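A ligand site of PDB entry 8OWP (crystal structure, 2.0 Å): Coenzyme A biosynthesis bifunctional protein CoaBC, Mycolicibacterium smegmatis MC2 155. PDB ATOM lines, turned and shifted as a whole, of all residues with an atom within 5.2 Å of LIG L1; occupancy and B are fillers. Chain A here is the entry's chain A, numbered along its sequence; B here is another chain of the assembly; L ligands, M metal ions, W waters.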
ATOM      1  N   GLY A  20      -6.942  24.203  26.145  1.00  0.00           N
ATOM      2  CA  GLY A  20      -7.076  24.118  27.583  1.00  0.00           C
ATOM      3  C   GLY A  20      -6.480  25.327  28.268  1.00  0.00           C
ATOM      4  O   GLY A  20      -6.053  26.292  27.631  1.00  0.00           O
ATOM      5  N   ASN A  34      -7.442  28.644  35.409  1.00  0.00           N
ATOM      6  CA  ASN A  34      -8.620  29.350  34.912  1.00  0.00           C
ATOM      7  C   ASN A  34      -9.674  28.321  34.515  1.00  0.00           C
ATOM      8  O   ASN A  34      -9.498  27.113  34.703  1.00  0.00           O
ATOM      9  CB  ASN A  34      -8.309  30.324  33.760  1.00  0.00           C
ATOM     10  CG  ASN A  34      -8.165  29.640  32.424  1.00  0.00           C
ATOM     11  OD1 ASN A  34      -7.812  28.477  32.328  1.00  0.00           O
ATOM     12  ND2 ASN A  34      -8.484  30.380  31.369  1.00  0.00           N
ATOM     13  N   SER A  36     -10.984  27.557  31.561  1.00  0.00           N
ATOM     14  CA  SER A  36     -10.988  27.081  30.175  1.00  0.00           C
ATOM     15  C   SER A  36     -11.168  25.570  30.075  1.00  0.00           C
ATOM     16  O   SER A  36     -10.387  24.790  30.651  1.00  0.00           O
ATOM     17  CB  SER A  36      -9.676  27.455  29.493  1.00  0.00           C
ATOM     18  OG  SER A  36      -9.542  28.852  29.420  1.00  0.00           O
ATOM     19  N   SER A  37     -12.148  25.129  29.279  1.00  0.00           N
ATOM     20  CA  SER A  37     -12.446  23.711  29.133  1.00  0.00           C
ATOM     21  C   SER A  37     -11.581  23.007  28.104  1.00  0.00           C
ATOM     22  O   SER A  37     -11.416  21.787  28.198  1.00  0.00           O
ATOM     23  CB  SER A  37     -13.910  23.520  28.735  1.00  0.00           C
ATOM     24  OG  SER A  37     -14.127  24.035  27.429  1.00  0.00           O
ATOM     25  N   GLY A  38     -11.033  23.735  27.134  1.00  0.00           N
ATOM     26  CA  GLY A  38     -10.306  23.191  26.008  1.00  0.00           C
ATOM     27  C   GLY A  38     -11.144  22.588  24.903  1.00  0.00           C
ATOM     28  O   GLY A  38     -10.585  22.164  23.895  1.00  0.00           O
ATOM     29  N   LYS A  39     -12.471  22.579  25.043  1.00  0.00           N
ATOM     30  CA  LYS A  39     -13.347  21.861  24.110  1.00  0.00           C
ATOM     31  C   LYS A  39     -13.254  22.395  22.688  1.00  0.00           C
ATOM     32  O   LYS A  39     -13.265  21.612  21.731  1.00  0.00           O
ATOM     33  CB  LYS A  39     -14.794  21.946  24.610  1.00  0.00           C
ATOM     34  CG  LYS A  39     -15.071  21.022  25.783  1.00  0.00           C
ATOM     35  CD  LYS A  39     -16.315  21.454  26.506  1.00  0.00           C
ATOM     36  CE  LYS A  39     -16.719  20.469  27.567  1.00  0.00           C
ATOM     37  NZ  LYS A  39     -18.067  20.869  28.044  1.00  0.00           N
ATOM     38  N   GLN A  40     -13.223  23.712  22.513  1.00  0.00           N
ATOM     39  CA  GLN A  40     -13.134  24.277  21.168  1.00  0.00           C
ATOM     40  C   GLN A  40     -11.768  24.001  20.560  1.00  0.00           C
ATOM     41  O   GLN A  40     -11.663  23.748  19.350  1.00  0.00           O
ATOM     42  CB  GLN A  40     -13.431  25.782  21.210  1.00  0.00           C
ATOM     43  CG  GLN A  40     -13.734  26.394  19.842  1.00  0.00           C
ATOM     44  CD  GLN A  40     -14.918  25.717  19.145  1.00  0.00           C
ATOM     45  OE1 GLN A  40     -16.081  25.981  19.452  1.00  0.00           O
ATOM     46  NE2 GLN A  40     -14.621  24.813  18.223  1.00  0.00           N
ATOM     47  N   GLY A  41     -10.716  24.031  21.367  1.00  0.00           N
ATOM     48  CA  GLY A  41      -9.393  23.726  20.873  1.00  0.00           C
ATOM     49  C   GLY A  41      -9.254  22.275  20.421  1.00  0.00           C
ATOM     50  O   GLY A  41      -8.651  22.003  19.379  1.00  0.00           O
ATOM     51  N   TYR A  42      -9.752  21.332  21.218  1.00  0.00           N
ATOM     52  CA  TYR A  42      -9.754  19.936  20.794  1.00  0.00           C
ATOM     53  C   TYR A  42     -10.587  19.740  19.520  1.00  0.00           C
ATOM     54  O   TYR A  42     -10.195  18.993  18.630  1.00  0.00           O
ATOM     55  CB  TYR A  42     -10.294  19.031  21.909  1.00  0.00           C
ATOM     56  CG  TYR A  42      -9.291  18.580  22.951  1.00  0.00           C
ATOM     57  CD1 TYR A  42      -8.457  19.486  23.606  1.00  0.00           C
ATOM     58  CD2 TYR A  42      -9.194  17.226  23.313  1.00  0.00           C
ATOM     59  CE1 TYR A  42      -7.554  19.077  24.566  1.00  0.00           C
ATOM     60  CE2 TYR A  42      -8.284  16.805  24.271  1.00  0.00           C
ATOM     61  CZ  TYR A  42      -7.474  17.733  24.897  1.00  0.00           C
ATOM     62  OH  TYR A  42      -6.561  17.322  25.857  1.00  0.00           O
ATOM     63  N   ALA A  99      -5.098  28.156  20.831  1.00  0.00           N
ATOM     64  CA  ALA A  99      -6.389  28.222  21.493  1.00  0.00           C
ATOM     65  C   ALA A  99      -6.278  28.132  23.000  1.00  0.00           C
ATOM     66  O   ALA A  99      -7.291  28.233  23.689  1.00  0.00           O
ATOM     67  CB  ALA A  99      -7.326  27.117  20.991  1.00  0.00           C
ATOM     68  N   ALA A 100      -5.080  27.909  23.525  1.00  0.00           N
ATOM     69  CA  ALA A 100      -4.903  27.782  24.960  1.00  0.00           C
ATOM     70  C   ALA A 100      -5.036  29.136  25.652  1.00  0.00           C
ATOM     71  O   ALA A 100      -4.636  30.166  25.105  1.00  0.00           O
ATOM     72  CB  ALA A 100      -3.555  27.145  25.279  1.00  0.00           C
ATOM     73  N   ALA A 101      -5.601  29.117  26.854  1.00  0.00           N
ATOM     74  CA  ALA A 101      -5.600  30.268  27.767  1.00  0.00           C
ATOM     75  C   ALA A 101      -4.288  30.222  28.542  1.00  0.00           C
ATOM     76  O   ALA A 101      -4.165  29.561  29.574  1.00  0.00           O
ATOM     77  CB  ALA A 101      -6.795  30.229  28.694  1.00  0.00           C
ATOM     78  N   VAL A 102      -3.280  30.864  28.001  1.00  0.00           N
ATOM     79  CA  VAL A 102      -1.955  30.845  28.608  1.00  0.00           C
ATOM     80  C   VAL A 102      -1.946  31.833  29.771  1.00  0.00           C
ATOM     81  O   VAL A 102      -2.309  33.005  29.603  1.00  0.00           O
ATOM     82  CB  VAL A 102      -0.876  31.160  27.554  1.00  0.00           C
ATOM     83  CG1 VAL A 102       0.501  30.949  28.094  1.00  0.00           C
ATOM     84  CG2 VAL A 102      -1.078  30.256  26.329  1.00  0.00           C
ATOM     85  N   PHE A 155      -6.594  32.949  19.625  1.00  0.00           N
ATOM     86  CA  PHE A 155      -7.937  32.933  20.179  1.00  0.00           C
ATOM     87  C   PHE A 155      -8.105  34.049  21.195  1.00  0.00           C
ATOM     88  O   PHE A 155      -7.143  34.482  21.826  1.00  0.00           O
ATOM     89  CB  PHE A 155      -8.254  31.622  20.871  1.00  0.00           C
ATOM     90  CG  PHE A 155      -8.715  30.567  19.947  1.00  0.00           C
ATOM     91  CD1 PHE A 155      -7.971  30.237  18.835  1.00  0.00           C
ATOM     92  CD2 PHE A 155      -9.905  29.907  20.166  1.00  0.00           C
ATOM     93  CE1 PHE A 155      -8.400  29.268  17.969  1.00  0.00           C
ATOM     94  CE2 PHE A 155     -10.335  28.937  19.309  1.00  0.00           C
ATOM     95  CZ  PHE A 155      -9.588  28.614  18.210  1.00  0.00           C
ATOM     96  N   ALA A 156      -9.330  34.515  21.346  1.00  0.00           N
ATOM     97  CA  ALA A 156      -9.634  35.549  22.319  1.00  0.00           C
ATOM     98  C   ALA A 156     -11.074  35.392  22.751  1.00  0.00           C
ATOM     99  O   ALA A 156     -11.937  35.002  21.962  1.00  0.00           O
ATOM    100  CB  ALA A 156      -9.388  36.954  21.738  1.00  0.00           C
ATOM    101  N   ALA A 157     -11.321  35.630  24.029  1.00  0.00           N
ATOM    102  CA  ALA A 157     -12.663  35.797  24.560  1.00  0.00           C
ATOM    103  C   ALA A 157     -12.756  37.256  24.956  1.00  0.00           C
ATOM    104  O   ALA A 157     -12.094  37.695  25.900  1.00  0.00           O
ATOM    105  CB  ALA A 157     -12.890  34.868  25.746  1.00  0.00           C
ATOM    106  N   VAL A 183      -9.585  34.189  16.279  1.00  0.00           N
ATOM    107  CA  VAL A 183     -10.882  33.550  16.483  1.00  0.00           C
ATOM    108  C   VAL A 183     -11.446  34.068  17.801  1.00  0.00           C
ATOM    109  O   VAL A 183     -10.954  33.728  18.882  1.00  0.00           O
ATOM    110  CB  VAL A 183     -10.759  32.022  16.485  1.00  0.00           C
ATOM    111  CG1 VAL A 183     -12.046  31.381  16.974  1.00  0.00           C
ATOM    112  CG2 VAL A 183     -10.378  31.513  15.104  1.00  0.00           C
ATOM    113  N   VAL A 184     -12.493  34.883  17.727  1.00  0.00           N
ATOM    114  CA  VAL A 184     -12.993  35.611  18.890  1.00  0.00           C
ATOM    115  C   VAL A 184     -14.353  35.070  19.288  1.00  0.00           C
ATOM    116  O   VAL A 184     -15.273  34.986  18.462  1.00  0.00           O
ATOM    117  CB  VAL A 184     -13.081  37.124  18.625  1.00  0.00           C
ATOM    118  CG1 VAL A 184     -13.552  37.857  19.892  1.00  0.00           C
ATOM    119  CG2 VAL A 184     -11.747  37.679  18.187  1.00  0.00           C
ATOM    120  N   ASN A 185     -14.489  34.735  20.544  1.00  0.00           N
ATOM    121  CA  ASN A 185     -15.777  34.429  21.106  1.00  0.00           C
ATOM    122  C   ASN A 185     -16.178  35.655  21.919  1.00  0.00           C
ATOM    123  O   ASN A 185     -15.325  36.416  22.360  1.00  0.00           O
ATOM    124  CB  ASN A 185     -15.692  33.162  21.938  1.00  0.00           C
ATOM    125  CG  ASN A 185     -16.955  32.853  22.654  1.00  0.00           C
ATOM    126  OD1 ASN A 185     -18.055  33.097  22.151  1.00  0.00           O
ATOM    127  ND2 ASN A 185     -16.820  32.289  23.835  1.00  0.00           N
ATOM    128  N   ASP A 199     -22.158  33.802  17.446  1.00  0.00           N
ATOM    129  CA  ASP A 199     -21.337  33.534  18.624  1.00  0.00           C
ATOM    130  C   ASP A 199     -20.113  34.431  18.739  1.00  0.00           C
ATOM    131  O   ASP A 199     -19.652  34.692  19.862  1.00  0.00           O
ATOM    132  CB  ASP A 199     -20.842  32.073  18.625  1.00  0.00           C
ATOM    133  CG  ASP A 199     -21.451  31.253  19.727  1.00  0.00           C
ATOM    134  OD1 ASP A 199     -22.386  31.739  20.381  1.00  0.00           O
ATOM    135  OD2 ASP A 199     -20.950  30.137  19.965  1.00  0.00           O
ATOM    136  N   LEU A 212     -18.995  34.450  13.701  1.00  0.00           N
ATOM    137  CA  LEU A 212     -18.956  33.024  13.966  1.00  0.00           C
ATOM    138  C   LEU A 212     -20.353  32.650  14.428  1.00  0.00           C
ATOM    139  O   LEU A 212     -20.785  33.057  15.515  1.00  0.00           O
ATOM    140  CB  LEU A 212     -17.895  32.705  15.003  1.00  0.00           C
ATOM    141  CG  LEU A 212     -17.497  31.238  15.066  1.00  0.00           C
ATOM    142  CD1 LEU A 212     -17.393  30.663  13.653  1.00  0.00           C
ATOM    143  CD2 LEU A 212     -16.200  31.067  15.861  1.00  0.00           C
ATOM    144  N   LYS A 217     -19.394  22.751  19.110  1.00  0.00           N
ATOM    145  CA  LYS A 217     -17.956  22.937  18.987  1.00  0.00           C
ATOM    146  C   LYS A 217     -17.418  22.293  17.709  1.00  0.00           C
ATOM    147  O   LYS A 217     -16.428  22.756  17.138  1.00  0.00           O
ATOM    148  CB  LYS A 217     -17.241  22.370  20.232  1.00  0.00           C
ATOM    149  CG  LYS A 217     -17.732  22.929  21.562  1.00  0.00           C
ATOM    150  CD  LYS A 217     -17.856  24.447  21.498  1.00  0.00           C
ATOM    151  CE  LYS A 217     -17.615  25.131  22.834  1.00  0.00           C
ATOM    152  NZ  LYS A 217     -17.410  26.581  22.591  1.00  0.00           N
ATOM    153  N   MET A 220     -18.528  24.733  14.779  1.00  0.00           N
ATOM    154  CA  MET A 220     -17.733  25.947  14.830  1.00  0.00           C
ATOM    155  C   MET A 220     -16.269  25.646  14.510  1.00  0.00           C
ATOM    156  O   MET A 220     -15.597  26.493  13.925  1.00  0.00           O
ATOM    157  CB  MET A 220     -17.892  26.654  16.179  1.00  0.00           C
ATOM    158  CG  MET A 220     -19.324  27.172  16.413  1.00  0.00           C
ATOM    159  SD  MET A 220     -19.492  28.331  17.772  1.00  0.00           S
ATOM    160  CE  MET A 220     -19.289  27.216  19.165  1.00  0.00           C
ATOM    161  N   ILE A 224     -14.032  27.408  11.419  1.00  0.00           N
ATOM    162  CA  ILE A 224     -12.688  27.897  11.692  1.00  0.00           C
ATOM    163  C   ILE A 224     -11.688  27.306  10.701  1.00  0.00           C
ATOM    164  O   ILE A 224     -10.964  28.030  10.019  1.00  0.00           O
ATOM    165  CB  ILE A 224     -12.310  27.565  13.141  1.00  0.00           C
ATOM    166  CG1 ILE A 224     -13.163  28.382  14.108  1.00  0.00           C
ATOM    167  CG2 ILE A 224     -10.847  27.808  13.364  1.00  0.00           C
ATOM    168  CD1 ILE A 224     -12.991  27.981  15.551  1.00  0.00           C
ATOM    169  N   LYS B 114     -12.480  40.204  34.552  1.00  0.00           N
ATOM    170  CA  LYS B 114     -11.209  39.547  34.222  1.00  0.00           C
ATOM    171  C   LYS B 114     -10.058  40.543  34.246  1.00  0.00           C
ATOM    172  O   LYS B 114     -10.157  41.648  33.692  1.00  0.00           O
ATOM    173  CB  LYS B 114     -11.312  38.866  32.837  1.00  0.00           C
ATOM    174  CG  LYS B 114      -9.975  38.614  32.089  1.00  0.00           C
ATOM    175  CD  LYS B 114     -10.171  37.971  30.692  1.00  0.00           C
ATOM    176  CE  LYS B 114      -8.968  38.223  29.739  1.00  0.00           C
ATOM    177  NZ  LYS B 114      -9.070  37.547  28.385  1.00  0.00           N
HETATM  178  C1  LIG L   1     -10.911  30.585  24.257  1.00  0.00           C
HETATM  179  C2  LIG L   1     -10.977  28.561  25.140  1.00  0.00           C
HETATM  180  C3  LIG L   1      -9.602  32.220  26.750  1.00  0.00           C
HETATM  181  C4  LIG L   1      -7.272  32.978  25.538  1.00  0.00           C
HETATM  182  C5  LIG L   1      -7.976  31.919  25.011  1.00  0.00           C
HETATM  183  C6  LIG L   1     -11.291  27.110  25.496  1.00  0.00           C
HETATM  184  C7  LIG L   1     -14.859  30.540  19.212  1.00  0.00           C
HETATM  185  C8  LIG L   1     -15.993  29.834  19.540  1.00  0.00           C
HETATM  186  C9  LIG L   1     -16.107  29.274  20.783  1.00  0.00           C
HETATM  187  C10 LIG L   1     -15.096  29.398  21.714  1.00  0.00           C
HETATM  188  C11 LIG L   1     -13.966  30.089  21.362  1.00  0.00           C
HETATM  189  C12 LIG L   1     -13.846  30.667  20.123  1.00  0.00           C
HETATM  190  C13 LIG L   1     -12.872  30.259  22.378  1.00  0.00           C
HETATM  191  C14 LIG L   1     -12.233  31.478  22.468  1.00  0.00           C
HETATM  192  C15 LIG L   1     -11.241  31.647  23.415  1.00  0.00           C
HETATM  193  C16 LIG L   1     -11.551  29.366  24.167  1.00  0.00           C
HETATM  194  C17 LIG L   1     -12.559  29.213  23.212  1.00  0.00           C
HETATM  195  C18 LIG L   1     -10.017  29.321  25.772  1.00  0.00           C
HETATM  196  C19 LIG L   1      -9.157  31.562  25.634  1.00  0.00           C
HETATM  197  C20 LIG L   1      -8.889  33.269  27.266  1.00  0.00           C
HETATM  198  C21 LIG L   1      -7.736  33.642  26.653  1.00  0.00           C
HETATM  199  C22 LIG L   1     -11.861  26.140  24.496  1.00  0.00           C
HETATM  200  N1  LIG L   1      -9.993  30.489  25.207  1.00  0.00           N
HETATM  201  O1  LIG L   1      -7.046  34.689  27.207  1.00  0.00           O
HETATM  202  O2  LIG L   1     -11.089  25.541  23.730  1.00  0.00           O
HETATM  203  O3  LIG L   1     -13.085  25.957  24.453  1.00  0.00           O
HETATM  204  O4  LIG L   1     -11.055  26.707  26.557  1.00  0.00           O
HETATM  205  N1  LG2 L   2      -1.300  34.020  24.694  1.00  0.00           N
HETATM  206  C1  LG2 L   2      -0.024  33.502  24.751  1.00  0.00           C
HETATM  207  N2  LG2 L   2       0.765  33.698  25.798  1.00  0.00           N
HETATM  208  C2  LG2 L   2       0.313  34.429  26.813  1.00  0.00           C
HETATM  209  C3  LG2 L   2      -0.960  34.964  26.768  1.00  0.00           C
HETATM  210  C4  LG2 L   2      -1.770  34.761  25.678  1.00  0.00           C
HETATM  211  O1  LG2 L   2       0.341  32.836  23.801  1.00  0.00           O
HETATM  212  N3  LG2 L   2       1.100  34.622  27.879  1.00  0.00           N
HETATM  213  C5  LG2 L   2      -2.039  33.722  23.493  1.00  0.00           C
HETATM  214  C6  LG2 L   2      -3.257  32.852  23.748  1.00  0.00           C
HETATM  215  O2  LG2 L   2      -3.040  31.504  23.369  1.00  0.00           O
HETATM  216  C7  LG2 L   2      -4.306  33.455  22.868  1.00  0.00           C
HETATM  217  C8  LG2 L   2      -3.825  34.832  22.494  1.00  0.00           C
HETATM  218  O3  LG2 L   2      -2.491  34.936  22.929  1.00  0.00           O
HETATM  219  O4  LG2 L   2      -4.340  32.780  21.642  1.00  0.00           O
HETATM  220  C9  LG2 L   2      -4.646  35.911  23.129  1.00  0.00           C
HETATM  221  O5  LG2 L   2      -4.807  35.647  24.496  1.00  0.00           O
HETATM  222  P1  LG2 L   2      -5.332  36.844  25.366  1.00  0.00           P
HETATM  223  O6  LG2 L   2      -6.655  37.059  24.779  1.00  0.00           O
HETATM  224  O7  LG2 L   2      -5.185  36.538  26.791  1.00  0.00           O
HETATM  225  O8  LG2 L   2      -4.313  37.996  25.018  1.00  0.00           O
HETATM  226  P2  LG2 L   2      -3.807  38.941  26.191  1.00  0.00           P
HETATM  227  O9  LG2 L   2      -2.942  39.987  25.551  1.00  0.00           O
HETATM  228  O10 LG2 L   2      -3.209  38.206  27.320  1.00  0.00           O
HETATM  229  O11 LG2 L   2      -5.217  39.522  26.631  1.00  0.00           O
HETATM  230  P3  LG2 L   2      -5.538  40.659  27.700  1.00  0.00           P
HETATM  231  O12 LG2 L   2      -6.915  40.957  27.264  1.00  0.00           O
HETATM  232  O13 LG2 L   2      -5.475  39.998  29.001  1.00  0.00           O
HETATM  233  O14 LG2 L   2      -4.526  41.721  27.449  1.00  0.00           O
HETATM  234 CA    CA M   1      -5.387  37.372  28.958  1.00  0.00          CA
HETATM  235  O   HOH W   1      -6.507  34.049  30.600  1.00  0.00           O
HETATM  236  O   HOH W   2      -8.455  25.964  24.621  1.00  0.00           O
HETATM  237  O   HOH W   3     -14.341  31.559  24.998  1.00  0.00           O
HETATM  238  O   HOH W   4      -4.337  33.524  27.162  1.00  0.00           O
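An oxygen (O6) of LG2 L2 lies within hydrogen-bond range of an oxygen (O1) of LIG L1, at 3.4 Å.
Water W2 lies within hydrogen-bond range of the backbone carbonyl oxygen (O) of Ala 99 (2.7 Å), the backbone NH (N) of Gly 20 (2.8 Å) and an oxygen (O2) of LIG L1 (2.8 Å). Water W4 lies within hydrogen-bond range of an oxygen (O1) of LIG L1 (2.9 Å), the backbone NH (N) of Val 102 (3.0 Å) and an oxygen (O5) of LG2 L2 (3.4 Å).
NE2 of Gln 40 lies within hydrogen-bond range of O of Lys 217. OG of Ser 36 sits at hydrogen-bond distance from ND2 of Asn 34 (2.7 Å). The side-chain hydroxyl (OG) of Ser 37 lies close to the backbone NH (N) of Lys 39. The backbone NH of Asn 185 is in hydrogen-bond range of the backbone carbonyl oxygen of Ala 156 (2.9 Å). OD1 of Asn 185 sits close to O of Asp 199 (3.2 Å). The backbone NH (N) of Ala 156 sits at hydrogen-bond distance from the backbone carbonyl oxygen (O) of Val 183, 3.1 Å away. The backbone carbonyl oxygen (O) of Leu 212 is in hydrogen-bond range of the backbone NH (N) of Asp 199, 2.5 Å away. N of Ala 101 is in hydrogen-bond range of O of Gly 20, at 3.0 Å.
Merely in contact with LIG L1: Ser 36 (3.3 Å), Lys 217 (3.5 Å), Asn 185 (3.6 Å), Ala 156 (3.6 Å), Ala 99 (3.6 Å), Phe 155 (3.6 Å), Leu 212 (3.6 Å), Val 183 (3.7 Å), Lys 114 of chain B (3.7 Å), Ala 100 (3.8 Å) and Ala 101 (3.9 Å). Hydrophobic or aromatic side chains that line LIG L1: Ala 101, Phe 155, Val 183 and Leu 212. Within 4 Å of LIG L1: Ser 36, Ser 37, Gly 38, Lys 39, Gln 40, Gly 41, Ala 99, Ala 100, Ala 101, Phe 155, Ala 156, Val 183, Asn 185, Leu 212, Lys 217 and Lys 114 of chain B. The nearest printed residue that does not touch LIG L1 is Ala 157 (4.03 Å).
The backbone NH of Gly 41 sits at hydrogen-bond distance from an oxygen (O2) of LIG L1, at 2.8 Å. N of Gln 40 is in hydrogen-bond range of O3 of LIG L1 (3.0 Å). An oxygen (O4) of LIG L1 sits at hydrogen-bond distance from the backbone NH of Gly 38 (3.0 Å). N of Ser 37 lies within hydrogen-bond range of O4 of LIG L1 (3.3 Å). The backbone NH (N) of Lys 39 lies within hydrogen-bond range of an oxygen (O3) of LIG L1, at 3.5 Å. O4 of LG2 L2 lies within hydrogen-bond range of N of Phe 155 (3.0 Å). The backbone carbonyl oxygen (O) of Phe 155 lies close to an oxygen (O4) of LG2 L2, 3.3 Å away. The backbone carbonyl oxygen (O) of Ala 100 is in hydrogen-bond range of an oxygen (O2) of LG2 L2 (2.7 Å).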
